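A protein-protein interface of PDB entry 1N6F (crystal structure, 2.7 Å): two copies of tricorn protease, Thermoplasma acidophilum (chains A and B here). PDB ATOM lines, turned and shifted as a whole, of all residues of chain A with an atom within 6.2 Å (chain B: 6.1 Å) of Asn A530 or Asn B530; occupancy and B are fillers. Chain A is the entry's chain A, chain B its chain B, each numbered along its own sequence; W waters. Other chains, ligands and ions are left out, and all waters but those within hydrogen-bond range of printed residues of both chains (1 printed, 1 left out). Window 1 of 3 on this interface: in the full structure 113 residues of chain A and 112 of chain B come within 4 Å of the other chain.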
ATOM      1  N   TYR A 475      18.134  13.735 -21.386  1.00  0.00           N
ATOM      2  CA  TYR A 475      17.684  14.063 -22.727  1.00  0.00           C
ATOM      3  C   TYR A 475      18.175  15.442 -23.170  1.00  0.00           C
ATOM      4  O   TYR A 475      18.427  16.330 -22.350  1.00  0.00           O
ATOM      5  CB  TYR A 475      16.143  13.978 -22.791  1.00  0.00           C
ATOM      6  CG  TYR A 475      15.596  12.566 -22.736  1.00  0.00           C
ATOM      7  CD1 TYR A 475      15.435  11.903 -21.534  1.00  0.00           C
ATOM      8  CD2 TYR A 475      15.289  11.878 -23.905  1.00  0.00           C
ATOM      9  CE1 TYR A 475      14.984  10.571 -21.493  1.00  0.00           C
ATOM     10  CE2 TYR A 475      14.833  10.549 -23.880  1.00  0.00           C
ATOM     11  CZ  TYR A 475      14.690   9.897 -22.667  1.00  0.00           C
ATOM     12  OH  TYR A 475      14.310   8.570 -22.649  1.00  0.00           O
ATOM     13  N   SER A 523       1.293   5.027 -29.234  1.00  0.00           N
ATOM     14  CA  SER A 523       0.839   4.030 -30.190  1.00  0.00           C
ATOM     15  C   SER A 523       1.109   2.734 -29.485  1.00  0.00           C
ATOM     16  O   SER A 523       2.169   2.540 -28.905  1.00  0.00           O
ATOM     17  CB  SER A 523       1.622   4.075 -31.468  1.00  0.00           C
ATOM     18  OG  SER A 523       1.545   5.363 -32.051  1.00  0.00           O
ATOM     19  N   PRO A 524       0.144   1.817 -29.524  1.00  0.00           N
ATOM     20  CA  PRO A 524       0.288   0.515 -28.851  1.00  0.00           C
ATOM     21  C   PRO A 524       1.268  -0.452 -29.514  1.00  0.00           C
ATOM     22  O   PRO A 524       1.365  -0.492 -30.736  1.00  0.00           O
ATOM     23  CB  PRO A 524      -1.139  -0.029 -28.874  1.00  0.00           C
ATOM     24  CG  PRO A 524      -1.632   0.436 -30.249  1.00  0.00           C
ATOM     25  CD  PRO A 524      -1.105   1.879 -30.318  1.00  0.00           C
ATOM     26  N   ASP A 525       1.989  -1.221 -28.703  1.00  0.00           N
ATOM     27  CA  ASP A 525       2.940  -2.218 -29.198  1.00  0.00           C
ATOM     28  C   ASP A 525       2.129  -3.487 -29.451  1.00  0.00           C
ATOM     29  O   ASP A 525       1.362  -3.898 -28.589  1.00  0.00           O
ATOM     30  CB  ASP A 525       4.045  -2.458 -28.143  1.00  0.00           C
ATOM     31  CG  ASP A 525       5.096  -3.482 -28.602  1.00  0.00           C
ATOM     32  OD1 ASP A 525       6.305  -3.230 -28.422  1.00  0.00           O
ATOM     33  OD2 ASP A 525       4.698  -4.543 -29.129  1.00  0.00           O
ATOM     34  N   ARG A 526       2.287  -4.117 -30.610  1.00  0.00           N
ATOM     35  CA  ARG A 526       1.482  -5.302 -30.896  1.00  0.00           C
ATOM     36  C   ARG A 526       1.933  -6.592 -30.273  1.00  0.00           C
ATOM     37  O   ARG A 526       1.234  -7.578 -30.355  1.00  0.00           O
ATOM     38  CB  ARG A 526       1.332  -5.503 -32.417  1.00  0.00           C
ATOM     39  CG  ARG A 526       0.781  -4.289 -33.180  1.00  0.00           C
ATOM     40  CD  ARG A 526      -0.576  -3.827 -32.652  1.00  0.00           C
ATOM     41  NE  ARG A 526      -1.057  -2.613 -33.321  1.00  0.00           N
ATOM     42  CZ  ARG A 526      -2.108  -1.892 -32.922  1.00  0.00           C
ATOM     43  NH1 ARG A 526      -2.468  -0.809 -33.585  1.00  0.00           N
ATOM     44  NH2 ARG A 526      -2.800  -2.238 -31.849  1.00  0.00           N
ATOM     45  N   VAL A 528       4.475  -6.759 -27.098  1.00  0.00           N
ATOM     46  CA  VAL A 528       4.782  -6.553 -25.675  1.00  0.00           C
ATOM     47  C   VAL A 528       3.933  -5.458 -25.056  1.00  0.00           C
ATOM     48  O   VAL A 528       3.628  -4.509 -25.739  1.00  0.00           O
ATOM     49  CB  VAL A 528       6.239  -6.117 -25.516  1.00  0.00           C
ATOM     50  CG1 VAL A 528       6.608  -6.134 -24.068  1.00  0.00           C
ATOM     51  CG2 VAL A 528       7.143  -7.014 -26.327  1.00  0.00           C
ATOM     52  N   LEU A 529       3.549  -5.579 -23.785  1.00  0.00           N
ATOM     53  CA  LEU A 529       2.786  -4.500 -23.162  1.00  0.00           C
ATOM     54  C   LEU A 529       3.693  -3.255 -23.167  1.00  0.00           C
ATOM     55  O   LEU A 529       4.614  -3.145 -22.368  1.00  0.00           O
ATOM     56  CB  LEU A 529       2.399  -4.849 -21.731  1.00  0.00           C
ATOM     57  CG  LEU A 529       1.798  -3.662 -20.952  1.00  0.00           C
ATOM     58  CD1 LEU A 529       0.565  -3.156 -21.686  1.00  0.00           C
ATOM     59  CD2 LEU A 529       1.424  -4.070 -19.508  1.00  0.00           C
ATOM     60  N   ASN A 530       3.439  -2.328 -24.078  1.00  0.00           N
ATOM     61  CA  ASN A 530       4.272  -1.140 -24.205  1.00  0.00           C
ATOM     62  C   ASN A 530       3.607  -0.121 -25.130  1.00  0.00           C
ATOM     63  O   ASN A 530       2.714  -0.472 -25.888  1.00  0.00           O
ATOM     64  CB  ASN A 530       5.631  -1.540 -24.810  1.00  0.00           C
ATOM     65  CG  ASN A 530       6.625  -0.384 -24.830  1.00  0.00           C
ATOM     66  OD1 ASN A 530       7.664  -0.463 -25.461  1.00  0.00           O
ATOM     67  ND2 ASN A 530       6.309   0.687 -24.113  1.00  0.00           N
ATOM     68  N   PHE A 531       4.055   1.129 -25.072  1.00  0.00           N
ATOM     69  CA  PHE A 531       3.545   2.157 -25.956  1.00  0.00           C
ATOM     70  C   PHE A 531       4.700   3.077 -26.267  1.00  0.00           C
ATOM     71  O   PHE A 531       5.629   3.170 -25.468  1.00  0.00           O
ATOM     72  CB  PHE A 531       2.425   2.941 -25.294  1.00  0.00           C
ATOM     73  CG  PHE A 531       1.264   2.096 -24.870  1.00  0.00           C
ATOM     74  CD1 PHE A 531       1.313   1.365 -23.691  1.00  0.00           C
ATOM     75  CD2 PHE A 531       0.132   2.020 -25.665  1.00  0.00           C
ATOM     76  CE1 PHE A 531       0.252   0.566 -23.309  1.00  0.00           C
ATOM     77  CE2 PHE A 531      -0.942   1.223 -25.296  1.00  0.00           C
ATOM     78  CZ  PHE A 531      -0.883   0.495 -24.115  1.00  0.00           C
ATOM     79  N   SER A 532       4.688   3.719 -27.436  1.00  0.00           N
ATOM     80  CA  SER A 532       5.769   4.661 -27.765  1.00  0.00           C
ATOM     81  C   SER A 532       5.224   5.760 -28.638  1.00  0.00           C
ATOM     82  O   SER A 532       4.133   5.619 -29.194  1.00  0.00           O
ATOM     83  CB  SER A 532       6.908   3.964 -28.500  1.00  0.00           C
ATOM     84  OG  SER A 532       6.644   3.862 -29.874  1.00  0.00           O
ATOM     85  N   PHE A 533       5.974   6.849 -28.773  1.00  0.00           N
ATOM     86  CA  PHE A 533       5.518   7.955 -29.622  1.00  0.00           C
ATOM     87  C   PHE A 533       5.971   7.812 -31.073  1.00  0.00           C
ATOM     88  O   PHE A 533       7.077   8.175 -31.420  1.00  0.00           O
ATOM     89  CB  PHE A 533       5.998   9.289 -29.061  1.00  0.00           C
ATOM     90  CG  PHE A 533       5.559   9.536 -27.659  1.00  0.00           C
ATOM     91  CD1 PHE A 533       6.447   9.396 -26.613  1.00  0.00           C
ATOM     92  CD2 PHE A 533       4.253   9.853 -27.375  1.00  0.00           C
ATOM     93  CE1 PHE A 533       6.038   9.560 -25.295  1.00  0.00           C
ATOM     94  CE2 PHE A 533       3.827  10.020 -26.050  1.00  0.00           C
ATOM     95  CZ  PHE A 533       4.727   9.871 -25.017  1.00  0.00           C
ATOM     96  N   TYR A 896      12.578 -10.091 -26.623  1.00  0.00           N
ATOM     97  CA  TYR A 896      11.173 -10.197 -26.440  1.00  0.00           C
ATOM     98  C   TYR A 896      10.574 -11.438 -27.078  1.00  0.00           C
ATOM     99  O   TYR A 896       9.553 -11.944 -26.616  1.00  0.00           O
ATOM    100  CB  TYR A 896      10.467  -8.950 -26.911  1.00  0.00           C
ATOM    101  CG  TYR A 896      10.725  -7.785 -26.022  1.00  0.00           C
ATOM    102  CD1 TYR A 896      11.518  -6.744 -26.452  1.00  0.00           C
ATOM    103  CD2 TYR A 896      10.238  -7.747 -24.732  1.00  0.00           C
ATOM    104  CE1 TYR A 896      11.839  -5.682 -25.622  1.00  0.00           C
ATOM    105  CE2 TYR A 896      10.544  -6.677 -23.871  1.00  0.00           C
ATOM    106  CZ  TYR A 896      11.341  -5.652 -24.327  1.00  0.00           C
ATOM    107  OH  TYR A 896      11.630  -4.581 -23.519  1.00  0.00           O
ATOM    108  N   LEU A 923      17.525  -1.010 -21.544  1.00  0.00           N
ATOM    109  CA  LEU A 923      16.121  -1.348 -21.718  1.00  0.00           C
ATOM    110  C   LEU A 923      15.876  -2.764 -21.247  1.00  0.00           C
ATOM    111  O   LEU A 923      14.826  -3.059 -20.700  1.00  0.00           O
ATOM    112  CB  LEU A 923      15.690  -1.189 -23.178  1.00  0.00           C
ATOM    113  CG  LEU A 923      16.023   0.184 -23.778  1.00  0.00           C
ATOM    114  CD1 LEU A 923      15.537   0.244 -25.236  1.00  0.00           C
ATOM    115  CD2 LEU A 923      15.401   1.281 -22.951  1.00  0.00           C
ATOM    116  N   LYS A 927      13.558  -4.342 -17.710  1.00  0.00           N
ATOM    117  CA  LYS A 927      12.561  -5.402 -17.613  1.00  0.00           C
ATOM    118  C   LYS A 927      12.937  -6.411 -16.540  1.00  0.00           C
ATOM    119  O   LYS A 927      12.133  -6.749 -15.697  1.00  0.00           O
ATOM    120  CB  LYS A 927      12.401  -6.129 -18.955  1.00  0.00           C
ATOM    121  CG  LYS A 927      11.135  -5.762 -19.720  1.00  0.00           C
ATOM    122  CD  LYS A 927      11.125  -4.286 -20.044  1.00  0.00           C
ATOM    123  CE  LYS A 927       9.888  -3.897 -20.798  1.00  0.00           C
ATOM    124  NZ  LYS A 927       9.905  -2.426 -21.009  1.00  0.00           N
ATOM    125  N   ASN A 949       5.486  -7.390 -17.372  1.00  0.00           N
ATOM    126  CA  ASN A 949       6.840  -7.675 -17.794  1.00  0.00           C
ATOM    127  C   ASN A 949       7.739  -7.911 -16.592  1.00  0.00           C
ATOM    128  O   ASN A 949       8.793  -7.300 -16.470  1.00  0.00           O
ATOM    129  CB  ASN A 949       7.376  -6.521 -18.627  1.00  0.00           C
ATOM    130  CG  ASN A 949       6.628  -6.363 -19.926  1.00  0.00           C
ATOM    131  OD1 ASN A 949       5.786  -5.489 -20.076  1.00  0.00           O
ATOM    132  ND2 ASN A 949       6.921  -7.233 -20.869  1.00  0.00           N
ATOM    133  N   TYR B 475       1.840 -13.196 -20.569  1.00  0.00           N
ATOM    134  CA  TYR B 475       1.280 -12.984 -21.875  1.00  0.00           C
ATOM    135  C   TYR B 475       0.450 -14.182 -22.311  1.00  0.00           C
ATOM    136  O   TYR B 475       0.664 -15.306 -21.859  1.00  0.00           O
ATOM    137  CB  TYR B 475       2.405 -12.691 -22.882  1.00  0.00           C
ATOM    138  CG  TYR B 475       3.042 -11.322 -22.726  1.00  0.00           C
ATOM    139  CD1 TYR B 475       4.028 -11.088 -21.779  1.00  0.00           C
ATOM    140  CD2 TYR B 475       2.612 -10.248 -23.490  1.00  0.00           C
ATOM    141  CE1 TYR B 475       4.570  -9.811 -21.588  1.00  0.00           C
ATOM    142  CE2 TYR B 475       3.147  -8.963 -23.310  1.00  0.00           C
ATOM    143  CZ  TYR B 475       4.122  -8.754 -22.351  1.00  0.00           C
ATOM    144  OH  TYR B 475       4.603  -7.475 -22.136  1.00  0.00           O
ATOM    145  N   SER B 523      10.610  -0.258 -33.808  1.00  0.00           N
ATOM    146  CA  SER B 523      10.463   1.075 -34.423  1.00  0.00           C
ATOM    147  C   SER B 523      10.876   2.020 -33.339  1.00  0.00           C
ATOM    148  O   SER B 523      10.476   1.881 -32.184  1.00  0.00           O
ATOM    149  CB  SER B 523       9.031   1.377 -34.834  1.00  0.00           C
ATOM    150  OG  SER B 523       8.544   0.388 -35.730  1.00  0.00           O
ATOM    151  N   PRO B 524      11.687   3.002 -33.689  1.00  0.00           N
ATOM    152  CA  PRO B 524      12.168   3.977 -32.706  1.00  0.00           C
ATOM    153  C   PRO B 524      11.124   4.978 -32.165  1.00  0.00           C
ATOM    154  O   PRO B 524      10.279   5.450 -32.908  1.00  0.00           O
ATOM    155  CB  PRO B 524      13.300   4.688 -33.476  1.00  0.00           C
ATOM    156  CG  PRO B 524      12.716   4.771 -34.855  1.00  0.00           C
ATOM    157  CD  PRO B 524      12.092   3.384 -35.051  1.00  0.00           C
ATOM    158  N   ASP B 525      11.181   5.293 -30.876  1.00  0.00           N
ATOM    159  CA  ASP B 525      10.279   6.273 -30.271  1.00  0.00           C
ATOM    160  C   ASP B 525      10.904   7.656 -30.537  1.00  0.00           C
ATOM    161  O   ASP B 525      12.103   7.858 -30.302  1.00  0.00           O
ATOM    162  CB  ASP B 525      10.172   6.009 -28.769  1.00  0.00           C
ATOM    163  CG  ASP B 525       9.226   7.001 -28.049  1.00  0.00           C
ATOM    164  OD1 ASP B 525       8.398   6.561 -27.220  1.00  0.00           O
ATOM    165  OD2 ASP B 525       9.321   8.214 -28.309  1.00  0.00           O
ATOM    166  N   ARG B 526      10.123   8.616 -31.017  1.00  0.00           N
ATOM    167  CA  ARG B 526      10.708   9.920 -31.337  1.00  0.00           C
ATOM    168  C   ARG B 526      10.937  10.871 -30.192  1.00  0.00           C
ATOM    169  O   ARG B 526      11.510  11.926 -30.395  1.00  0.00           O
ATOM    170  CB  ARG B 526       9.874  10.643 -32.406  1.00  0.00           C
ATOM    171  CG  ARG B 526       9.636   9.832 -33.694  1.00  0.00           C
ATOM    172  CD  ARG B 526      10.930   9.416 -34.392  1.00  0.00           C
ATOM    173  NE  ARG B 526      10.696   8.581 -35.571  1.00  0.00           N
ATOM    174  CZ  ARG B 526      11.647   7.900 -36.215  1.00  0.00           C
ATOM    175  NH1 ARG B 526      11.345   7.165 -37.267  1.00  0.00           N
ATOM    176  NH2 ARG B 526      12.906   7.938 -35.811  1.00  0.00           N
ATOM    177  N   VAL B 528      11.117   9.612 -26.296  1.00  0.00           N
ATOM    178  CA  VAL B 528      11.785   8.900 -25.217  1.00  0.00           C
ATOM    179  C   VAL B 528      12.680   7.778 -25.729  1.00  0.00           C
ATOM    180  O   VAL B 528      12.355   7.180 -26.742  1.00  0.00           O
ATOM    181  CB  VAL B 528      10.728   8.250 -24.311  1.00  0.00           C
ATOM    182  CG1 VAL B 528      11.382   7.722 -23.072  1.00  0.00           C
ATOM    183  CG2 VAL B 528       9.626   9.231 -23.992  1.00  0.00           C
ATOM    184  N   LEU B 529      13.784   7.479 -25.038  1.00  0.00           N
ATOM    185  CA  LEU B 529      14.620   6.377 -25.488  1.00  0.00           C
ATOM    186  C   LEU B 529      13.781   5.108 -25.324  1.00  0.00           C
ATOM    187  O   LEU B 529      13.592   4.626 -24.212  1.00  0.00           O
ATOM    188  CB  LEU B 529      15.870   6.259 -24.650  1.00  0.00           C
ATOM    189  CG  LEU B 529      16.672   4.970 -24.895  1.00  0.00           C
ATOM    190  CD1 LEU B 529      17.055   4.911 -26.357  1.00  0.00           C
ATOM    191  CD2 LEU B 529      17.942   4.922 -23.999  1.00  0.00           C
ATOM    192  N   ASN B 530      13.266   4.570 -26.427  1.00  0.00           N
ATOM    193  CA  ASN B 530      12.395   3.399 -26.370  1.00  0.00           C
ATOM    194  C   ASN B 530      12.160   2.857 -27.768  1.00  0.00           C
ATOM    195  O   ASN B 530      12.366   3.555 -28.727  1.00  0.00           O
ATOM    196  CB  ASN B 530      11.032   3.813 -25.785  1.00  0.00           C
ATOM    197  CG  ASN B 530      10.127   2.614 -25.495  1.00  0.00           C
ATOM    198  OD1 ASN B 530       8.941   2.767 -25.236  1.00  0.00           O
ATOM    199  ND2 ASN B 530      10.697   1.414 -25.525  1.00  0.00           N
ATOM    200  N   PHE B 531      11.703   1.618 -27.873  1.00  0.00           N
ATOM    201  CA  PHE B 531      11.384   1.028 -29.164  1.00  0.00           C
ATOM    202  C   PHE B 531      10.183   0.118 -28.958  1.00  0.00           C
ATOM    203  O   PHE B 531       9.980  -0.406 -27.857  1.00  0.00           O
ATOM    204  CB  PHE B 531      12.558   0.212 -29.713  1.00  0.00           C
ATOM    205  CG  PHE B 531      13.819   1.013 -29.902  1.00  0.00           C
ATOM    206  CD1 PHE B 531      14.670   1.261 -28.816  1.00  0.00           C
ATOM    207  CD2 PHE B 531      14.136   1.545 -31.150  1.00  0.00           C
ATOM    208  CE1 PHE B 531      15.799   2.014 -28.957  1.00  0.00           C
ATOM    209  CE2 PHE B 531      15.280   2.314 -31.314  1.00  0.00           C
ATOM    210  CZ  PHE B 531      16.120   2.552 -30.211  1.00  0.00           C
ATOM    211  N   SER B 532       9.357  -0.054 -29.987  1.00  0.00           N
ATOM    212  CA  SER B 532       8.223  -0.977 -29.850  1.00  0.00           C
ATOM    213  C   SER B 532       7.926  -1.625 -31.172  1.00  0.00           C
ATOM    214  O   SER B 532       8.387  -1.148 -32.207  1.00  0.00           O
ATOM    215  CB  SER B 532       6.975  -0.256 -29.394  1.00  0.00           C
ATOM    216  OG  SER B 532       6.367   0.418 -30.462  1.00  0.00           O
ATOM    217  N   TYR B 896       5.762  11.499 -19.622  1.00  0.00           N
ATOM    218  CA  TYR B 896       6.950  11.726 -20.389  1.00  0.00           C
ATOM    219  C   TYR B 896       7.142  13.177 -20.795  1.00  0.00           C
ATOM    220  O   TYR B 896       8.265  13.642 -20.986  1.00  0.00           O
ATOM    221  CB  TYR B 896       7.012  10.806 -21.602  1.00  0.00           C
ATOM    222  CG  TYR B 896       7.234   9.384 -21.217  1.00  0.00           C
ATOM    223  CD1 TYR B 896       6.211   8.463 -21.336  1.00  0.00           C
ATOM    224  CD2 TYR B 896       8.442   8.964 -20.674  1.00  0.00           C
ATOM    225  CE1 TYR B 896       6.375   7.146 -20.924  1.00  0.00           C
ATOM    226  CE2 TYR B 896       8.622   7.638 -20.249  1.00  0.00           C
ATOM    227  CZ  TYR B 896       7.587   6.736 -20.379  1.00  0.00           C
ATOM    228  OH  TYR B 896       7.746   5.418 -19.994  1.00  0.00           O
ATOM    229  N   LEU B 923       4.133   0.673 -16.042  1.00  0.00           N
ATOM    230  CA  LEU B 923       5.120   1.218 -16.947  1.00  0.00           C
ATOM    231  C   LEU B 923       5.805   2.397 -16.295  1.00  0.00           C
ATOM    232  O   LEU B 923       6.994   2.626 -16.495  1.00  0.00           O
ATOM    233  CB  LEU B 923       4.478   1.639 -18.276  1.00  0.00           C
ATOM    234  CG  LEU B 923       3.662   0.527 -18.947  1.00  0.00           C
ATOM    235  CD1 LEU B 923       3.078   1.029 -20.258  1.00  0.00           C
ATOM    236  CD2 LEU B 923       4.513  -0.704 -19.163  1.00  0.00           C
ATOM    237  N   LYS B 927      10.001   2.989 -14.838  1.00  0.00           N
ATOM    238  CA  LYS B 927      10.949   4.070 -15.071  1.00  0.00           C
ATOM    239  C   LYS B 927      11.500   4.602 -13.759  1.00  0.00           C
ATOM    240  O   LYS B 927      12.690   4.750 -13.607  1.00  0.00           O
ATOM    241  CB  LYS B 927      10.281   5.218 -15.843  1.00  0.00           C
ATOM    242  CG  LYS B 927      10.697   5.315 -17.297  1.00  0.00           C
ATOM    243  CD  LYS B 927      10.322   4.051 -18.031  1.00  0.00           C
ATOM    244  CE  LYS B 927      10.741   4.108 -19.477  1.00  0.00           C
ATOM    245  NZ  LYS B 927      10.380   2.812 -20.125  1.00  0.00           N
ATOM    246  N   ASN B 949      16.721   6.770 -18.806  1.00  0.00           N
ATOM    247  CA  ASN B 949      15.473   7.010 -18.118  1.00  0.00           C
ATOM    248  C   ASN B 949      15.618   6.696 -16.636  1.00  0.00           C
ATOM    249  O   ASN B 949      14.866   5.883 -16.085  1.00  0.00           O
ATOM    250  CB  ASN B 949      14.373   6.159 -18.729  1.00  0.00           C
ATOM    251  CG  ASN B 949      14.094   6.532 -20.147  1.00  0.00           C
ATOM    252  OD1 ASN B 949      14.535   5.870 -21.076  1.00  0.00           O
ATOM    253  ND2 ASN B 949      13.368   7.616 -20.331  1.00  0.00           N
HETATM  254  O   HOH W   1       9.598   0.581 -22.227  1.00  0.00           O
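The side-chain hydroxyl (OH) of Tyr A475 is in hydrogen-bond range of the backbone NH (N) of Leu B529, at 2.7 Å. The side-chain hydroxyl (OH) of Tyr A475 is in hydrogen-bond range of the side-chain amide nitrogen (ND2) of Asn B949, at 2.7 Å. N of Leu A529 sits at hydrogen-bond distance from OH of Tyr B475 (2.7 Å). OD1 of Asn A530 lies close to OD1 of Asn B530 (3.5 Å). The side-chain amide oxygen of Asn A530 sits close to the backbone carbonyl oxygen of Phe B531. O of Phe A531 sits close to OD1 of Asn B530 (3.3 Å). The side-chain carboxylate (OD1) of Asp B525 lies within hydrogen-bond range of the backbone NH (N) of Phe A533 (2.9 Å). The backbone carbonyl oxygen (O) of Phe A533 sits at hydrogen-bond distance from the backbone NH (N) of Arg B526, at 3.1 Å. The side-chain amide nitrogen (ND2) of Asn A949 is in hydrogen-bond range of the side-chain hydroxyl (OH) of Tyr B475.
N of Ser A523 is in hydrogen-bond range of O of Ser A532 (2.9 Å). N of Asp A525 lies within hydrogen-bond range of O of Asn A530 (3.0 Å). OD1 of Asn A949 lies close to O of Leu A529. The backbone NH (N) of Ser B523 sits at hydrogen-bond distance from the backbone carbonyl oxygen (O) of Ser B532 (2.9 Å). The backbone NH of Val B528 sits at hydrogen-bond distance from the side-chain carboxylate of Asp B525 (3.0 Å). N of Asp B525 lies within hydrogen-bond range of O of Asn B530, 3.0 Å away.
Val B528 touches Tyr A475 (CG1 to OH, 3.1 Å). CB of Ser B532 touches OD1 of Asp A525 (3.2 Å). Val A528 touches Tyr B475 (CG1 to OH, 3.1 Å). Asn A530 touches Ser B532 (OD1 to CB, 3.998 Å). Phe A531 touches Leu B923. Ser A532 touches Asp B525 (CB to OD1, 3.3 Å). OG of Ser A532 touches OG of Ser B532, 3.5 Å away. CG2 of Val B528 touches CE1 of Phe A533, 3.8 Å away. Phe B531 touches Leu A923.
Of the printed residues of chain B, Asn A530 touches Asn B530 (3.5 Å), Phe B531 (3.3 Å) and Ser B532 (3.998 Å). Of chain A, only Asn A530 (3.5 Å) and Phe A531 (3.3 Å) come within 4 Å of Asn B530. Printed residues of chain B within 4 Å of Phe A531: Asn B530 and Leu B923. Printed residues of chain A within 4 Å of Leu B529: Tyr A475 (2.7 Å). Lys A927 touches none of the printed residues of chain B. Pro B524 touches none of the printed residues of chain A. The nearest printed residue of chain B that does not touch Tyr A475 is Asn B530 (5.6 Å).
Of the 14 printed residues of chain B, 10 touch a printed residue of chain A. Hydrophobic or aromatic side chains of chain B within 4 Å of the printed part of chain A: Tyr B475, Val B528, Leu B529, Phe B531 and Leu B923. Among the printed residues, 18 pairs touch across the chains. Among the printed residues, no Asp or Glu carboxylate lies within 4 Å of a Lys or Arg side-chain nitrogen of the other chain.
Tyr A475 touches Leu B529, and with the chains exchanged Leu A529 touches Tyr B475. Asp A525 touches Ser B532, and with the chains exchanged Ser A532 touches Asp B525. Phe A531 touches Leu B923, and with the chains exchanged Leu A923 touches Phe B531. Ser A532 touches its own counterpart, Ser B532.
Water W1 lies within hydrogen-bond range of NZ of Lys B927 (3.2 Å) and NZ of Lys A927 (3.3 Å).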
